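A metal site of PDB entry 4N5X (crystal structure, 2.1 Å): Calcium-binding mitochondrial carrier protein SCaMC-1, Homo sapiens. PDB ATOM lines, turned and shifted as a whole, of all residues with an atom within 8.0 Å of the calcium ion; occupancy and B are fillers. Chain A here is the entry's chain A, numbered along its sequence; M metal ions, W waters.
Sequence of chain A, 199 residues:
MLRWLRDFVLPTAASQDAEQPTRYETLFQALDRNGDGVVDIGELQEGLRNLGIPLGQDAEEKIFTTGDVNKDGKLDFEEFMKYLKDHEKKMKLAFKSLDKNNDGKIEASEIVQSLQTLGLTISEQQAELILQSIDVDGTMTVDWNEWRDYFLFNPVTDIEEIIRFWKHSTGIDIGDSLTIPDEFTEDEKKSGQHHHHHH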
ATOM      1  N   LYS A 105      17.035 -19.943 -15.389  1.00  0.00           N
ATOM      2  CA  LYS A 105      16.326 -19.211 -16.426  1.00  0.00           C
ATOM      3  C   LYS A 105      17.175 -19.083 -17.684  1.00  0.00           C
ATOM      4  O   LYS A 105      18.386 -19.018 -17.613  1.00  0.00           O
ATOM      5  CB  LYS A 105      15.933 -17.808 -15.942  1.00  0.00           C
ATOM      6  CG  LYS A 105      15.089 -17.766 -14.668  1.00  0.00           C
ATOM      7  CD  LYS A 105      13.656 -18.198 -14.940  1.00  0.00           C
ATOM      8  CE  LYS A 105      12.983 -18.728 -13.667  1.00  0.00           C
ATOM      9  NZ  LYS A 105      13.005 -17.739 -12.551  1.00  0.00           N
ATOM     10  N   ILE A 106      16.530 -19.024 -18.850  1.00  0.00           N
ATOM     11  CA  ILE A 106      17.256 -18.699 -20.077  1.00  0.00           C
ATOM     12  C   ILE A 106      16.908 -17.299 -20.566  1.00  0.00           C
ATOM     13  O   ILE A 106      15.738 -16.954 -20.727  1.00  0.00           O
ATOM     14  CB  ILE A 106      17.000 -19.759 -21.186  1.00  0.00           C
ATOM     15  CG1 ILE A 106      17.499 -21.139 -20.749  1.00  0.00           C
ATOM     16  CG2 ILE A 106      17.675 -19.351 -22.500  1.00  0.00           C
ATOM     17  CD1 ILE A 106      16.994 -22.259 -21.629  1.00  0.00           C
ATOM     18  N   LEU A 131      13.145 -16.328 -27.849  1.00  0.00           N
ATOM     19  CA  LEU A 131      12.597 -16.084 -26.517  1.00  0.00           C
ATOM     20  C   LEU A 131      11.101 -15.811 -26.559  1.00  0.00           C
ATOM     21  O   LEU A 131      10.327 -16.350 -25.756  1.00  0.00           O
ATOM     22  CB  LEU A 131      13.303 -14.890 -25.860  1.00  0.00           C
ATOM     23  CG  LEU A 131      14.539 -15.177 -25.021  1.00  0.00           C
ATOM     24  CD1 LEU A 131      14.847 -13.965 -24.189  1.00  0.00           C
ATOM     25  CD2 LEU A 131      14.341 -16.376 -24.128  1.00  0.00           C
ATOM     26  N   ILE A 134       8.604 -18.778 -26.821  1.00  0.00           N
ATOM     27  CA  ILE A 134       8.476 -19.688 -25.685  1.00  0.00           C
ATOM     28  C   ILE A 134       7.974 -18.985 -24.409  1.00  0.00           C
ATOM     29  O   ILE A 134       7.250 -19.566 -23.593  1.00  0.00           O
ATOM     30  CB  ILE A 134       9.827 -20.397 -25.423  1.00  0.00           C
ATOM     31  CG1 ILE A 134      10.195 -21.270 -26.625  1.00  0.00           C
ATOM     32  CG2 ILE A 134       9.749 -21.249 -24.170  1.00  0.00           C
ATOM     33  CD1 ILE A 134      11.691 -21.679 -26.693  1.00  0.00           C
ATOM     34  N   ASP A 135       8.347 -17.714 -24.269  1.00  0.00           N
ATOM     35  CA  ASP A 135       7.989 -16.910 -23.104  1.00  0.00           C
ATOM     36  C   ASP A 135       6.488 -16.638 -23.059  1.00  0.00           C
ATOM     37  O   ASP A 135       5.944 -15.931 -23.909  1.00  0.00           O
ATOM     38  CB  ASP A 135       8.759 -15.590 -23.137  1.00  0.00           C
ATOM     39  CG  ASP A 135       8.540 -14.741 -21.885  1.00  0.00           C
ATOM     40  OD1 ASP A 135       8.218 -15.314 -20.845  1.00  0.00           O
ATOM     41  OD2 ASP A 135       8.702 -13.520 -21.958  1.00  0.00           O
ATOM     42  N   VAL A 136       5.805 -17.191 -22.069  1.00  0.00           N
ATOM     43  CA  VAL A 136       4.355 -17.029 -22.011  1.00  0.00           C
ATOM     44  C   VAL A 136       3.904 -15.904 -21.065  1.00  0.00           C
ATOM     45  O   VAL A 136       2.906 -15.254 -21.320  1.00  0.00           O
ATOM     46  CB  VAL A 136       3.616 -18.350 -21.704  1.00  0.00           C
ATOM     47  CG1 VAL A 136       3.667 -18.676 -20.228  1.00  0.00           C
ATOM     48  CG2 VAL A 136       2.171 -18.256 -22.160  1.00  0.00           C
ATOM     49  N   ASP A 137       4.659 -15.643 -20.002  1.00  0.00           N
ATOM     50  CA  ASP A 137       4.276 -14.593 -19.051  1.00  0.00           C
ATOM     51  C   ASP A 137       4.961 -13.246 -19.303  1.00  0.00           C
ATOM     52  O   ASP A 137       4.869 -12.323 -18.480  1.00  0.00           O
ATOM     53  CB  ASP A 137       4.491 -15.059 -17.617  1.00  0.00           C
ATOM     54  CG  ASP A 137       5.918 -15.477 -17.349  1.00  0.00           C
ATOM     55  OD1 ASP A 137       6.766 -15.234 -18.225  1.00  0.00           O
ATOM     56  OD2 ASP A 137       6.208 -16.028 -16.261  1.00  0.00           O
ATOM     57  N   GLY A 138       5.654 -13.121 -20.432  1.00  0.00           N
ATOM     58  CA  GLY A 138       6.322 -11.880 -20.800  1.00  0.00           C
ATOM     59  C   GLY A 138       7.474 -11.395 -19.931  1.00  0.00           C
ATOM     60  O   GLY A 138       7.720 -10.191 -19.852  1.00  0.00           O
ATOM     61  N   THR A 139       8.195 -12.307 -19.297  1.00  0.00           N
ATOM     62  CA  THR A 139       9.343 -11.907 -18.469  1.00  0.00           C
ATOM     63  C   THR A 139      10.604 -11.723 -19.310  1.00  0.00           C
ATOM     64  O   THR A 139      11.613 -11.208 -18.825  1.00  0.00           O
ATOM     65  CB  THR A 139       9.647 -12.945 -17.372  1.00  0.00           C
ATOM     66  OG1 THR A 139       9.828 -14.233 -17.981  1.00  0.00           O
ATOM     67  CG2 THR A 139       8.514 -13.029 -16.367  1.00  0.00           C
ATOM     68  N   MET A 140      10.542 -12.142 -20.574  1.00  0.00           N
ATOM     69  CA  MET A 140      11.718 -12.205 -21.443  1.00  0.00           C
ATOM     70  C   MET A 140      12.785 -13.126 -20.841  1.00  0.00           C
ATOM     71  O   MET A 140      13.977 -12.990 -21.108  1.00  0.00           O
ATOM     72  CB  MET A 140      12.276 -10.808 -21.788  1.00  0.00           C
ATOM     73  CG  MET A 140      11.433 -10.048 -22.820  1.00  0.00           C
ATOM     74  SD  MET A 140      11.125 -10.966 -24.374  1.00  0.00           S
ATOM     75  CE  MET A 140      12.763 -10.970 -25.132  1.00  0.00           C
ATOM     76  N   THR A 141      12.326 -14.053 -20.023  1.00  0.00           N
ATOM     77  CA  THR A 141      13.155 -15.116 -19.493  1.00  0.00           C
ATOM     78  C   THR A 141      12.330 -16.378 -19.671  1.00  0.00           C
ATOM     79  O   THR A 141      11.128 -16.341 -19.510  1.00  0.00           O
ATOM     80  CB  THR A 141      13.452 -14.922 -17.997  1.00  0.00           C
ATOM     81  OG1 THR A 141      12.230 -14.944 -17.254  1.00  0.00           O
ATOM     82  CG2 THR A 141      14.148 -13.576 -17.753  1.00  0.00           C
ATOM     83  N   VAL A 142      12.972 -17.485 -20.021  1.00  0.00           N
ATOM     84  CA  VAL A 142      12.242 -18.738 -20.160  1.00  0.00           C
ATOM     85  C   VAL A 142      12.497 -19.593 -18.939  1.00  0.00           C
ATOM     86  O   VAL A 142      13.649 -19.874 -18.625  1.00  0.00           O
ATOM     87  CB  VAL A 142      12.673 -19.528 -21.417  1.00  0.00           C
ATOM     88  CG1 VAL A 142      12.138 -20.965 -21.375  1.00  0.00           C
ATOM     89  CG2 VAL A 142      12.249 -18.797 -22.687  1.00  0.00           C
ATOM     90  N   ASP A 143      11.438 -20.002 -18.247  1.00  0.00           N
ATOM     91  CA  ASP A 143      11.598 -20.869 -17.078  1.00  0.00           C
ATOM     92  C   ASP A 143      11.359 -22.325 -17.489  1.00  0.00           C
ATOM     93  O   ASP A 143      10.914 -22.594 -18.605  1.00  0.00           O
ATOM     94  CB  ASP A 143      10.679 -20.439 -15.930  1.00  0.00           C
ATOM     95  CG  ASP A 143       9.212 -20.474 -16.308  1.00  0.00           C
ATOM     96  OD1 ASP A 143       8.791 -21.370 -17.055  1.00  0.00           O
ATOM     97  OD2 ASP A 143       8.459 -19.583 -15.847  1.00  0.00           O
ATOM     98  N   TRP A 144      11.641 -23.247 -16.580  1.00  0.00           N
ATOM     99  CA  TRP A 144      11.580 -24.660 -16.926  1.00  0.00           C
ATOM    100  C   TRP A 144      10.200 -25.089 -17.439  1.00  0.00           C
ATOM    101  O   TRP A 144      10.122 -25.822 -18.423  1.00  0.00           O
ATOM    102  CB  TRP A 144      12.013 -25.538 -15.750  1.00  0.00           C
ATOM    103  CG  TRP A 144      11.608 -26.983 -15.883  1.00  0.00           C
ATOM    104  CD1 TRP A 144      10.758 -27.675 -15.070  1.00  0.00           C
ATOM    105  CD2 TRP A 144      12.011 -27.910 -16.896  1.00  0.00           C
ATOM    106  NE1 TRP A 144      10.622 -28.971 -15.502  1.00  0.00           N
ATOM    107  CE2 TRP A 144      11.388 -29.134 -16.619  1.00  0.00           C
ATOM    108  CE3 TRP A 144      12.870 -27.811 -18.003  1.00  0.00           C
ATOM    109  CZ2 TRP A 144      11.572 -30.262 -17.419  1.00  0.00           C
ATOM    110  CZ3 TRP A 144      13.051 -28.948 -18.801  1.00  0.00           C
ATOM    111  CH2 TRP A 144      12.402 -30.155 -18.498  1.00  0.00           C
ATOM    112  N   GLU A 146       7.874 -23.283 -18.969  1.00  0.00           N
ATOM    113  CA  GLU A 146       7.697 -22.734 -20.298  1.00  0.00           C
ATOM    114  C   GLU A 146       8.458 -23.540 -21.338  1.00  0.00           C
ATOM    115  O   GLU A 146       7.926 -23.857 -22.398  1.00  0.00           O
ATOM    116  CB  GLU A 146       8.164 -21.277 -20.341  1.00  0.00           C
ATOM    117  CG  GLU A 146       7.297 -20.306 -19.539  1.00  0.00           C
ATOM    118  CD  GLU A 146       7.838 -18.883 -19.535  1.00  0.00           C
ATOM    119  OE1 GLU A 146       9.080 -18.713 -19.429  1.00  0.00           O
ATOM    120  OE2 GLU A 146       7.025 -17.939 -19.638  1.00  0.00           O
ATOM    121  N   TRP A 147       9.714 -23.851 -21.043  1.00  0.00           N
ATOM    122  CA  TRP A 147      10.572 -24.644 -21.923  1.00  0.00           C
ATOM    123  C   TRP A 147      10.002 -26.055 -22.145  1.00  0.00           C
ATOM    124  O   TRP A 147       9.818 -26.505 -23.291  1.00  0.00           O
ATOM    125  CB  TRP A 147      11.951 -24.757 -21.275  1.00  0.00           C
ATOM    126  CG  TRP A 147      12.964 -25.569 -22.012  1.00  0.00           C
ATOM    127  CD1 TRP A 147      13.240 -26.888 -21.825  1.00  0.00           C
ATOM    128  CD2 TRP A 147      13.885 -25.108 -23.020  1.00  0.00           C
ATOM    129  NE1 TRP A 147      14.257 -27.285 -22.659  1.00  0.00           N
ATOM    130  CE2 TRP A 147      14.677 -26.212 -23.397  1.00  0.00           C
ATOM    131  CE3 TRP A 147      14.107 -23.870 -23.626  1.00  0.00           C
ATOM    132  CZ2 TRP A 147      15.669 -26.110 -24.365  1.00  0.00           C
ATOM    133  CZ3 TRP A 147      15.099 -23.769 -24.594  1.00  0.00           C
ATOM    134  CH2 TRP A 147      15.870 -24.882 -24.953  1.00  0.00           C
HETATM  135 CA    CA M   1       8.815 -16.290 -18.933  1.00  0.00          CA
HETATM  136  O   HOH W   1       8.683 -17.061 -16.627  1.00  0.00           O
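N of Gly 138 lies close to OD2 of Asp 135.
N of Met 140 lies within hydrogen-bond range of OD2 of Asp 135.
OE2 of Glu 146 lies close to N of Val 136, 2.8 Å away.
The backbone NH (N) of Glu 146 lies within hydrogen-bond range of the side-chain carboxylate (OD1) of Asp 143 (2.9 Å).
Of the 16 residues printed, 5 come within 4 Å of the calcium ion.
The nearest printed residue that does not touch the calcium ion is Val 142 (4.4 Å).
The calcium ion is bound by OD1 of Asp 135, O of Thr 141, OD1 of Asp 137, water W1, OG1 of Thr 139, OE1 of Glu 146 and OE2 of Glu 146.
Water W1 lies within hydrogen-bond range of the side-chain carboxylate (OD2) of Asp 143 (2.6 Å) and the side-chain carboxylate (OD2) of Asp 137 (2.7 Å).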
